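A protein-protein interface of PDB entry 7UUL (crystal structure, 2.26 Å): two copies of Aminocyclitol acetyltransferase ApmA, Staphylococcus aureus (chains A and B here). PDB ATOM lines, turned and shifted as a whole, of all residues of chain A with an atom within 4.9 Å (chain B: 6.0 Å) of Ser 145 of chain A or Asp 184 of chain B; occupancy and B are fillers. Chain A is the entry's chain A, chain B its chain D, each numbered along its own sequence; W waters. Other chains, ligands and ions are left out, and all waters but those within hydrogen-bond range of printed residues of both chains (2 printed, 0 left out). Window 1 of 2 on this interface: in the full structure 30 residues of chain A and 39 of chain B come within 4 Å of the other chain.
N of Ser 145 of chain A is in hydrogen-bond range of OD1 of Asp 184 of chain B. OD2 of Asp 184 of chain B sits close to O of Thr 142 of chain A (3.5 Å). The backbone carbonyl oxygen (O) of Asp 147 of chain A sits close to the side-chain amide oxygen (OE1) of Gln 102 of chain B (3.4 Å). N of Val 144 of chain A lies within hydrogen-bond range of OD1 of Asp 184 of chain B, 2.6 Å away. N of Val 144 of chain A lies close to NH2 of Arg 234 of chain B (3.3 Å). The backbone carbonyl oxygen (O) of Thr 142 of chain A is in hydrogen-bond range of the guanidinium group (NH2) of Arg 234 of chain B (3.0 Å).
Of chain B, only Phe 124 (3.1 Å) and Asp 184 (3.0 Å) come within 4 Å of Ser 145 of chain A. Of the printed residues of chain B, Asp 146 of chain A touches Ser 126 (3.6 Å). Of the printed residues of chain A, Ser 126 of chain B touches His 137 (3.98 Å) and Asp 146 (3.6 Å). Gly 182 of chain B touches none of the printed residues of chain A. Of chain A, only Thr 142 (3.5 Å), Phe 143 (3.3 Å), Val 144 (2.6 Å) and Ser 145 (3.0 Å) come within 4 Å of Asp 184 of chain B. The nearest printed residue of chain A that does not touch Asp 184 of chain B is Gln 138 of chain A (6.0 Å). The nearest printed residue of chain A that does not touch Tyr 186 of chain B is Val 144 of chain A (4.04 Å).
Hydrophobic or aromatic side chains of chain A within 4 Å of the printed part of chain B: His 137, Phe 143, Val 144 and Ile 148. Among the printed residues, 16 pairs touch across the chains. Among the printed residues, no Asp or Glu carboxylate lies within 4 Å of a Lys or Arg side-chain nitrogen of the other chain.
No position is printed for both chains. Of the 16 pairs that touch across the chains among the printed residues, none has its exchanged pair printed and touching as well.
NE2 of Gln 138 of chain A lies within hydrogen-bond range of O of Ser 145 of chain A (3.1 Å). O of Val 144 of chain A lies within hydrogen-bond range of ND1 of His 137 of chain A (2.8 Å). NE2 of Gln 138 of chain A lies close to O of Val 144 of chain A (3.4 Å). NH1 of Arg 234 of chain B is in hydrogen-bond range of O of Gly 204 of chain B (2.9 Å). The backbone carbonyl oxygen (O) of Ala 205 of chain B lies within hydrogen-bond range of the backbone NH (N) of Tyr 186 of chain B (3.0 Å). OD2 of Asp 184 of chain B lies within salt-bridge range of NH1 of Arg 234 of chain B (3.0 Å).
Water W1 lies within hydrogen-bond range of the backbone carbonyl oxygen of Thr 142 of chain A (2.7 Å), the side-chain carboxylate of Asp 184 of chain B (2.8 Å) and the indole nitrogen of Trp 248 of chain B (2.9 Å). Water W2 lies within hydrogen-bond range of OG of Ser 145 of chain A, OG of Ser 126 of chain B, O of Gln 102 of chain B and N of Asp 147 of chain A.
Among the printed residues, pairs that only touch across the chains: His 137 of chain A with Ser 126 of chain B (3.98 Å), His 137 of chain A with Tyr 186 of chain B (3.5 Å), Thr 142 of chain A with Phe 235 of chain B (3.3 Å), Phe 143 of chain A with Asp 184 of chain B (3.3 Å), Phe 143 of chain A with Arg 234 of chain B (3.4 Å), Phe 143 of chain A with Trp 248 of chain B (3.3 Å), Ser 145 of chain A with Phe 124 of chain B (3.1 Å), Asp 146 of chain A with Ser 126 of chain B (3.6 Å), Ile 148 of chain A with Phe 124 of chain B (3.6 Å) and Ile 148 of chain A with Trp 248 of chain B (3.6 Å).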
ATOM      1  N   HIS A 137       2.287  -2.039 -22.961  1.00  0.00           N
ATOM      2  CA  HIS A 137       3.637  -1.494 -22.982  1.00  0.00           C
ATOM      3  C   HIS A 137       3.705  -0.340 -23.972  1.00  0.00           C
ATOM      4  O   HIS A 137       2.755  -0.070 -24.707  1.00  0.00           O
ATOM      5  CB  HIS A 137       4.658  -2.568 -23.341  1.00  0.00           C
ATOM      6  CG  HIS A 137       4.802  -3.619 -22.293  1.00  0.00           C
ATOM      7  ND1 HIS A 137       5.757  -4.610 -22.355  1.00  0.00           N
ATOM      8  CD2 HIS A 137       4.102  -3.834 -21.153  1.00  0.00           C
ATOM      9  CE1 HIS A 137       5.643  -5.390 -21.296  1.00  0.00           C
ATOM     10  NE2 HIS A 137       4.643  -4.943 -20.552  1.00  0.00           N
ATOM     11  N   GLN A 138       4.838   0.360 -23.984  1.00  0.00           N
ATOM     12  CA  GLN A 138       5.006   1.428 -24.960  1.00  0.00           C
ATOM     13  C   GLN A 138       4.861   0.854 -26.363  1.00  0.00           C
ATOM     14  O   GLN A 138       5.355  -0.238 -26.661  1.00  0.00           O
ATOM     15  CB  GLN A 138       6.367   2.123 -24.802  1.00  0.00           C
ATOM     16  CG  GLN A 138       7.581   1.297 -25.244  1.00  0.00           C
ATOM     17  CD  GLN A 138       7.965   0.223 -24.221  1.00  0.00           C
ATOM     18  OE1 GLN A 138       7.539   0.270 -23.062  1.00  0.00           O
ATOM     19  NE2 GLN A 138       8.787  -0.741 -24.647  1.00  0.00           N
ATOM     20  N   THR A 142      11.133   1.429 -30.593  1.00  0.00           N
ATOM     21  CA  THR A 142      11.606   0.315 -31.406  1.00  0.00           C
ATOM     22  C   THR A 142      11.350  -1.022 -30.717  1.00  0.00           C
ATOM     23  O   THR A 142      11.062  -2.019 -31.383  1.00  0.00           O
ATOM     24  CB  THR A 142      13.091   0.519 -31.713  1.00  0.00           C
ATOM     25  OG1 THR A 142      13.255   1.793 -32.350  1.00  0.00           O
ATOM     26  CG2 THR A 142      13.634  -0.564 -32.628  1.00  0.00           C
ATOM     27  N   PHE A 143      11.431  -1.049 -29.393  1.00  0.00           N
ATOM     28  CA  PHE A 143      11.173  -2.231 -28.598  1.00  0.00           C
ATOM     29  C   PHE A 143       9.840  -2.089 -27.874  1.00  0.00           C
ATOM     30  O   PHE A 143       9.343  -0.980 -27.646  1.00  0.00           O
ATOM     31  CB  PHE A 143      12.299  -2.470 -27.573  1.00  0.00           C
ATOM     32  CG  PHE A 143      12.434  -1.364 -26.552  1.00  0.00           C
ATOM     33  CD1 PHE A 143      13.106  -0.183 -26.865  1.00  0.00           C
ATOM     34  CD2 PHE A 143      11.867  -1.493 -25.289  1.00  0.00           C
ATOM     35  CE1 PHE A 143      13.220   0.848 -25.928  1.00  0.00           C
ATOM     36  CE2 PHE A 143      11.963  -0.463 -24.358  1.00  0.00           C
ATOM     37  CZ  PHE A 143      12.639   0.707 -24.671  1.00  0.00           C
ATOM     38  N   VAL A 144       9.273  -3.241 -27.527  1.00  0.00           N
ATOM     39  CA  VAL A 144       8.043  -3.330 -26.744  1.00  0.00           C
ATOM     40  C   VAL A 144       8.283  -3.929 -25.365  1.00  0.00           C
ATOM     41  O   VAL A 144       7.408  -3.813 -24.491  1.00  0.00           O
ATOM     42  CB  VAL A 144       6.963  -4.133 -27.500  1.00  0.00           C
ATOM     43  CG1 VAL A 144       7.306  -5.617 -27.535  1.00  0.00           C
ATOM     44  CG2 VAL A 144       5.567  -3.879 -26.936  1.00  0.00           C
ATOM     45  N   SER A 145       9.449  -4.529 -25.135  1.00  0.00           N
ATOM     46  CA  SER A 145       9.776  -5.153 -23.860  1.00  0.00           C
ATOM     47  C   SER A 145       9.742  -4.141 -22.716  1.00  0.00           C
ATOM     48  O   SER A 145       9.997  -2.947 -22.903  1.00  0.00           O
ATOM     49  CB  SER A 145      11.167  -5.791 -23.952  1.00  0.00           C
ATOM     50  OG  SER A 145      11.703  -6.046 -22.664  1.00  0.00           O
ATOM     51  N   ASP A 146       9.434  -4.626 -21.513  1.00  0.00           N
ATOM     52  CA  ASP A 146       9.641  -3.810 -20.322  1.00  0.00           C
ATOM     53  C   ASP A 146      10.891  -4.196 -19.540  1.00  0.00           C
ATOM     54  O   ASP A 146      11.594  -3.322 -19.038  1.00  0.00           O
ATOM     55  CB  ASP A 146       8.416  -3.856 -19.401  1.00  0.00           C
ATOM     56  CG  ASP A 146       8.186  -5.223 -18.774  1.00  0.00           C
ATOM     57  OD1 ASP A 146       8.596  -6.215 -19.401  1.00  0.00           O
ATOM     58  OD2 ASP A 146       7.564  -5.305 -17.681  1.00  0.00           O
ATOM     59  N   ASP A 147      11.226  -5.471 -19.440  1.00  0.00           N
ATOM     60  CA  ASP A 147      12.361  -5.822 -18.597  1.00  0.00           C
ATOM     61  C   ASP A 147      13.694  -5.490 -19.241  1.00  0.00           C
ATOM     62  O   ASP A 147      14.726  -5.540 -18.561  1.00  0.00           O
ATOM     63  CB  ASP A 147      12.294  -7.303 -18.204  1.00  0.00           C
ATOM     64  CG  ASP A 147      11.353  -7.534 -17.027  1.00  0.00           C
ATOM     65  OD1 ASP A 147      10.850  -6.527 -16.478  1.00  0.00           O
ATOM     66  OD2 ASP A 147      11.112  -8.702 -16.650  1.00  0.00           O
ATOM     67  N   ILE A 148      13.698  -5.127 -20.526  1.00  0.00           N
ATOM     68  CA  ILE A 148      14.896  -4.531 -21.116  1.00  0.00           C
ATOM     69  C   ILE A 148      15.448  -3.428 -20.218  1.00  0.00           C
ATOM     70  O   ILE A 148      16.669  -3.279 -20.080  1.00  0.00           O
ATOM     71  CB  ILE A 148      14.588  -4.015 -22.541  1.00  0.00           C
ATOM     72  CG1 ILE A 148      15.871  -3.536 -23.231  1.00  0.00           C
ATOM     73  CG2 ILE A 148      13.515  -2.934 -22.499  1.00  0.00           C
ATOM     74  CD1 ILE A 148      15.659  -2.966 -24.622  1.00  0.00           C
ATOM     75  N   TYR A 172       1.929   1.478 -19.404  1.00  0.00           N
ATOM     76  CA  TYR A 172       2.043   1.170 -17.979  1.00  0.00           C
ATOM     77  C   TYR A 172       1.092   2.036 -17.162  1.00  0.00           C
ATOM     78  O   TYR A 172       1.348   2.325 -15.991  1.00  0.00           O
ATOM     79  CB  TYR A 172       3.493   1.334 -17.494  1.00  0.00           C
ATOM     80  CG  TYR A 172       4.479   0.644 -18.405  1.00  0.00           C
ATOM     81  CD1 TYR A 172       4.665  -0.734 -18.320  1.00  0.00           C
ATOM     82  CD2 TYR A 172       5.219   1.356 -19.363  1.00  0.00           C
ATOM     83  CE1 TYR A 172       5.542  -1.402 -19.155  1.00  0.00           C
ATOM     84  CE2 TYR A 172       6.126   0.687 -20.202  1.00  0.00           C
ATOM     85  CZ  TYR A 172       6.263  -0.702 -20.091  1.00  0.00           C
ATOM     86  OH  TYR A 172       7.120  -1.423 -20.887  1.00  0.00           O
ATOM     87  N   GLN B 102      15.958 -11.386 -20.001  1.00  0.00           N
ATOM     88  CA  GLN B 102      14.836 -10.506 -19.682  1.00  0.00           C
ATOM     89  C   GLN B 102      13.536 -10.971 -20.334  1.00  0.00           C
ATOM     90  O   GLN B 102      12.671 -10.160 -20.677  1.00  0.00           O
ATOM     91  CB  GLN B 102      15.130  -9.051 -20.074  1.00  0.00           C
ATOM     92  CG  GLN B 102      16.438  -8.499 -19.557  1.00  0.00           C
ATOM     93  CD  GLN B 102      16.547  -8.559 -18.046  1.00  0.00           C
ATOM     94  OE1 GLN B 102      15.551  -8.549 -17.335  1.00  0.00           O
ATOM     95  NE2 GLN B 102      17.771  -8.609 -17.551  1.00  0.00           N
ATOM     96  N   GLY B 122      12.801 -16.037 -27.444  1.00  0.00           N
ATOM     97  CA  GLY B 122      13.768 -14.993 -27.694  1.00  0.00           C
ATOM     98  C   GLY B 122      14.093 -14.137 -26.484  1.00  0.00           C
ATOM     99  O   GLY B 122      13.719 -14.403 -25.334  1.00  0.00           O
ATOM    100  N   GLN B 123      14.831 -13.071 -26.778  1.00  0.00           N
ATOM    101  CA  GLN B 123      15.263 -12.107 -25.786  1.00  0.00           C
ATOM    102  C   GLN B 123      14.219 -11.004 -25.627  1.00  0.00           C
ATOM    103  O   GLN B 123      13.559 -10.610 -26.589  1.00  0.00           O
ATOM    104  CB  GLN B 123      16.595 -11.475 -26.191  1.00  0.00           C
ATOM    105  CG  GLN B 123      17.597 -12.370 -26.895  1.00  0.00           C
ATOM    106  CD  GLN B 123      18.880 -12.486 -26.112  1.00  0.00           C
ATOM    107  OE1 GLN B 123      18.857 -12.558 -24.879  1.00  0.00           O
ATOM    108  NE2 GLN B 123      20.012 -12.418 -26.811  1.00  0.00           N
ATOM    109  N   PHE B 124      14.093 -10.494 -24.397  1.00  0.00           N
ATOM    110  CA  PHE B 124      13.257  -9.329 -24.094  1.00  0.00           C
ATOM    111  C   PHE B 124      11.811  -9.582 -24.488  1.00  0.00           C
ATOM    112  O   PHE B 124      11.104  -8.689 -24.961  1.00  0.00           O
ATOM    113  CB  PHE B 124      13.817  -8.066 -24.762  1.00  0.00           C
ATOM    114  CG  PHE B 124      15.261  -7.809 -24.408  1.00  0.00           C
ATOM    115  CD1 PHE B 124      15.605  -7.403 -23.124  1.00  0.00           C
ATOM    116  CD2 PHE B 124      16.283  -8.041 -25.338  1.00  0.00           C
ATOM    117  CE1 PHE B 124      16.950  -7.193 -22.773  1.00  0.00           C
ATOM    118  CE2 PHE B 124      17.615  -7.841 -24.999  1.00  0.00           C
ATOM    119  CZ  PHE B 124      17.955  -7.408 -23.711  1.00  0.00           C
ATOM    120  N   THR B 125      11.367 -10.812 -24.273  1.00  0.00           N
ATOM    121  CA  THR B 125      10.026 -11.242 -24.621  1.00  0.00           C
ATOM    122  C   THR B 125       9.175 -11.342 -23.357  1.00  0.00           C
ATOM    123  O   THR B 125       9.646 -11.810 -22.316  1.00  0.00           O
ATOM    124  CB  THR B 125      10.093 -12.572 -25.378  1.00  0.00           C
ATOM    125  OG1 THR B 125      10.568 -12.318 -26.712  1.00  0.00           O
ATOM    126  CG2 THR B 125       8.730 -13.271 -25.432  1.00  0.00           C
ATOM    127  N   SER B 126       7.925 -10.893 -23.457  1.00  0.00           N
ATOM    128  CA  SER B 126       7.058 -10.662 -22.309  1.00  0.00           C
ATOM    129  C   SER B 126       5.733 -11.379 -22.541  1.00  0.00           C
ATOM    130  O   SER B 126       4.951 -10.987 -23.417  1.00  0.00           O
ATOM    131  CB  SER B 126       6.827  -9.173 -22.099  1.00  0.00           C
ATOM    132  OG  SER B 126       8.030  -8.439 -22.224  1.00  0.00           O
ATOM    133  N   GLY B 182       9.843 -15.442 -30.979  1.00  0.00           N
ATOM    134  CA  GLY B 182      10.904 -14.484 -31.215  1.00  0.00           C
ATOM    135  C   GLY B 182      11.201 -13.561 -30.036  1.00  0.00           C
ATOM    136  O   GLY B 182      10.658 -13.667 -28.931  1.00  0.00           O
ATOM    137  N   SER B 183      12.124 -12.648 -30.299  1.00  0.00           N
ATOM    138  CA  SER B 183      12.540 -11.628 -29.352  1.00  0.00           C
ATOM    139  C   SER B 183      11.652 -10.398 -29.492  1.00  0.00           C
ATOM    140  O   SER B 183      11.040 -10.163 -30.537  1.00  0.00           O
ATOM    141  CB  SER B 183      14.007 -11.242 -29.581  1.00  0.00           C
ATOM    142  OG  SER B 183      14.882 -12.361 -29.575  1.00  0.00           O
ATOM    143  N   ASP B 184      11.596  -9.602 -28.417  1.00  0.00           N
ATOM    144  CA  ASP B 184      10.763  -8.395 -28.363  1.00  0.00           C
ATOM    145  C   ASP B 184       9.320  -8.728 -28.706  1.00  0.00           C
ATOM    146  O   ASP B 184       8.624  -7.939 -29.357  1.00  0.00           O
ATOM    147  CB  ASP B 184      11.293  -7.282 -29.283  1.00  0.00           C
ATOM    148  CG  ASP B 184      10.691  -5.908 -28.959  1.00  0.00           C
ATOM    149  OD1 ASP B 184      10.448  -5.603 -27.747  1.00  0.00           O
ATOM    150  OD2 ASP B 184      10.458  -5.137 -29.931  1.00  0.00           O
ATOM    151  N   VAL B 185       8.888  -9.936 -28.282  1.00  0.00           N
ATOM    152  CA  VAL B 185       7.519 -10.406 -28.450  1.00  0.00           C
ATOM    153  C   VAL B 185       6.713 -10.044 -27.205  1.00  0.00           C
ATOM    154  O   VAL B 185       7.231 -10.056 -26.080  1.00  0.00           O
ATOM    155  CB  VAL B 185       7.495 -11.925 -28.721  1.00  0.00           C
ATOM    156  CG1 VAL B 185       6.131 -12.524 -28.357  1.00  0.00           C
ATOM    157  CG2 VAL B 185       7.806 -12.200 -30.174  1.00  0.00           C
ATOM    158  N   TYR B 186       5.443  -9.707 -27.407  1.00  0.00           N
ATOM    159  CA  TYR B 186       4.532  -9.389 -26.321  1.00  0.00           C
ATOM    160  C   TYR B 186       3.251 -10.194 -26.488  1.00  0.00           C
ATOM    161  O   TYR B 186       2.616 -10.136 -27.543  1.00  0.00           O
ATOM    162  CB  TYR B 186       4.205  -7.898 -26.306  1.00  0.00           C
ATOM    163  CG  TYR B 186       3.273  -7.532 -25.196  1.00  0.00           C
ATOM    164  CD1 TYR B 186       1.897  -7.661 -25.339  1.00  0.00           C
ATOM    165  CD2 TYR B 186       3.766  -7.088 -23.977  1.00  0.00           C
ATOM    166  CE1 TYR B 186       1.028  -7.342 -24.287  1.00  0.00           C
ATOM    167  CE2 TYR B 186       2.916  -6.746 -22.939  1.00  0.00           C
ATOM    168  CZ  TYR B 186       1.551  -6.883 -23.101  1.00  0.00           C
ATOM    169  OH  TYR B 186       0.716  -6.544 -22.071  1.00  0.00           O
ATOM    170  N   ASP B 203       9.759 -12.610 -34.501  1.00  0.00           N
ATOM    171  CA  ASP B 203      10.374 -11.508 -33.767  1.00  0.00           C
ATOM    172  C   ASP B 203       9.483 -10.275 -33.798  1.00  0.00           C
ATOM    173  O   ASP B 203       9.012  -9.873 -34.864  1.00  0.00           O
ATOM    174  CB  ASP B 203      11.736 -11.164 -34.396  1.00  0.00           C
ATOM    175  CG  ASP B 203      12.818 -12.220 -34.114  1.00  0.00           C
ATOM    176  OD1 ASP B 203      12.883 -12.770 -32.981  1.00  0.00           O
ATOM    177  OD2 ASP B 203      13.608 -12.492 -35.037  1.00  0.00           O
ATOM    178  N   GLY B 204       9.254  -9.676 -32.622  1.00  0.00           N
ATOM    179  CA  GLY B 204       8.525  -8.418 -32.529  1.00  0.00           C
ATOM    180  C   GLY B 204       7.012  -8.505 -32.612  1.00  0.00           C
ATOM    181  O   GLY B 204       6.347  -7.468 -32.507  1.00  0.00           O
ATOM    182  N   ALA B 205       6.442  -9.695 -32.775  1.00  0.00           N
ATOM    183  CA  ALA B 205       4.989  -9.839 -32.806  1.00  0.00           C
ATOM    184  C   ALA B 205       4.361  -9.449 -31.477  1.00  0.00           C
ATOM    185  O   ALA B 205       4.924  -9.673 -30.397  1.00  0.00           O
ATOM    186  CB  ALA B 205       4.590 -11.279 -33.126  1.00  0.00           C
ATOM    187  N   ILE B 206       3.159  -8.892 -31.565  1.00  0.00           N
ATOM    188  CA  ILE B 206       2.314  -8.631 -30.408  1.00  0.00           C
ATOM    189  C   ILE B 206       1.077  -9.508 -30.529  1.00  0.00           C
ATOM    190  O   ILE B 206       0.362  -9.453 -31.539  1.00  0.00           O
ATOM    191  CB  ILE B 206       1.910  -7.151 -30.316  1.00  0.00           C
ATOM    192  CG1 ILE B 206       3.142  -6.255 -30.175  1.00  0.00           C
ATOM    193  CG2 ILE B 206       0.979  -6.939 -29.146  1.00  0.00           C
ATOM    194  CD1 ILE B 206       2.783  -4.755 -30.142  1.00  0.00           C
ATOM    195  N   PHE B 220       6.725  -8.830 -36.249  1.00  0.00           N
ATOM    196  CA  PHE B 220       6.194  -7.492 -35.970  1.00  0.00           C
ATOM    197  C   PHE B 220       4.718  -7.331 -36.338  1.00  0.00           C
ATOM    198  O   PHE B 220       4.200  -6.196 -36.344  1.00  0.00           O
ATOM    199  CB  PHE B 220       7.060  -6.412 -36.636  1.00  0.00           C
ATOM    200  CG  PHE B 220       8.450  -6.392 -36.084  1.00  0.00           C
ATOM    201  CD1 PHE B 220       8.717  -5.743 -34.888  1.00  0.00           C
ATOM    202  CD2 PHE B 220       9.467  -7.109 -36.697  1.00  0.00           C
ATOM    203  CE1 PHE B 220       9.996  -5.774 -34.324  1.00  0.00           C
ATOM    204  CE2 PHE B 220      10.751  -7.138 -36.142  1.00  0.00           C
ATOM    205  CZ  PHE B 220      11.015  -6.475 -34.950  1.00  0.00           C
ATOM    206  N   ARG B 234       3.859  -3.320 -36.454  1.00  0.00           N
ATOM    207  CA  ARG B 234       4.440  -2.266 -35.625  1.00  0.00           C
ATOM    208  C   ARG B 234       5.265  -1.276 -36.443  1.00  0.00           C
ATOM    209  O   ARG B 234       5.355  -0.096 -36.081  1.00  0.00           O
ATOM    210  CB  ARG B 234       5.308  -2.890 -34.526  1.00  0.00           C
ATOM    211  CG  ARG B 234       4.538  -3.678 -33.487  1.00  0.00           C
ATOM    212  CD  ARG B 234       5.470  -4.429 -32.575  1.00  0.00           C
ATOM    213  NE  ARG B 234       6.465  -3.573 -31.938  1.00  0.00           N
ATOM    214  CZ  ARG B 234       7.552  -4.029 -31.322  1.00  0.00           C
ATOM    215  NH1 ARG B 234       7.826  -5.322 -31.273  1.00  0.00           N
ATOM    216  NH2 ARG B 234       8.384  -3.163 -30.743  1.00  0.00           N
ATOM    217  N   PHE B 235       5.880  -1.732 -37.537  1.00  0.00           N
ATOM    218  CA  PHE B 235       6.813  -0.909 -38.289  1.00  0.00           C
ATOM    219  C   PHE B 235       6.607  -1.123 -39.783  1.00  0.00           C
ATOM    220  O   PHE B 235       5.985  -2.099 -40.220  1.00  0.00           O
ATOM    221  CB  PHE B 235       8.273  -1.216 -37.913  1.00  0.00           C
ATOM    222  CG  PHE B 235       8.560  -1.077 -36.445  1.00  0.00           C
ATOM    223  CD1 PHE B 235       8.467   0.162 -35.816  1.00  0.00           C
ATOM    224  CD2 PHE B 235       8.928  -2.184 -35.693  1.00  0.00           C
ATOM    225  CE1 PHE B 235       8.727   0.304 -34.450  1.00  0.00           C
ATOM    226  CE2 PHE B 235       9.203  -2.063 -34.342  1.00  0.00           C
ATOM    227  CZ  PHE B 235       9.095  -0.812 -33.709  1.00  0.00           C
ATOM    228  N   TRP B 248      18.824  -6.188 -32.560  1.00  0.00           N
ATOM    229  CA  TRP B 248      19.284  -5.462 -31.379  1.00  0.00           C
ATOM    230  C   TRP B 248      19.134  -6.310 -30.129  1.00  0.00           C
ATOM    231  O   TRP B 248      19.868  -6.111 -29.153  1.00  0.00           O
ATOM    232  CB  TRP B 248      18.534  -4.128 -31.206  1.00  0.00           C
ATOM    233  CG  TRP B 248      17.053  -4.265 -30.949  1.00  0.00           C
ATOM    234  CD1 TRP B 248      16.053  -4.112 -31.859  1.00  0.00           C
ATOM    235  CD2 TRP B 248      16.408  -4.580 -29.699  1.00  0.00           C
ATOM    236  NE1 TRP B 248      14.828  -4.315 -31.264  1.00  0.00           N
ATOM    237  CE2 TRP B 248      15.022  -4.612 -29.941  1.00  0.00           C
ATOM    238  CE3 TRP B 248      16.871  -4.848 -28.406  1.00  0.00           C
ATOM    239  CZ2 TRP B 248      14.099  -4.901 -28.944  1.00  0.00           C
ATOM    240  CZ3 TRP B 248      15.959  -5.139 -27.419  1.00  0.00           C
ATOM    241  CH2 TRP B 248      14.586  -5.156 -27.687  1.00  0.00           C
ATOM    242  N   TRP B 249      18.194  -7.257 -30.132  1.00  0.00           N
ATOM    243  CA  TRP B 249      17.954  -8.037 -28.923  1.00  0.00           C
ATOM    244  C   TRP B 249      19.126  -8.941 -28.562  1.00  0.00           C
ATOM    245  O   TRP B 249      19.151  -9.465 -27.445  1.00  0.00           O
ATOM    246  CB  TRP B 249      16.680  -8.859 -29.094  1.00  0.00           C
ATOM    247  CG  TRP B 249      16.537  -9.366 -30.505  1.00  0.00           C
ATOM    248  CD1 TRP B 249      17.150 -10.463 -31.048  1.00  0.00           C
ATOM    249  CD2 TRP B 249      15.762  -8.777 -31.562  1.00  0.00           C
ATOM    250  NE1 TRP B 249      16.791 -10.601 -32.368  1.00  0.00           N
ATOM    251  CE2 TRP B 249      15.937  -9.581 -32.707  1.00  0.00           C
ATOM    252  CE3 TRP B 249      14.929  -7.654 -31.645  1.00  0.00           C
ATOM    253  CZ2 TRP B 249      15.302  -9.300 -33.927  1.00  0.00           C
ATOM    254  CZ3 TRP B 249      14.301  -7.377 -32.848  1.00  0.00           C
ATOM    255  CH2 TRP B 249      14.496  -8.196 -33.980  1.00  0.00           C
HETATM  256  O   HOH W   1      12.074  -4.410 -32.068  1.00  0.00           O
HETATM  257  O   HOH W   2      10.663  -8.258 -21.363  1.00  0.00           O
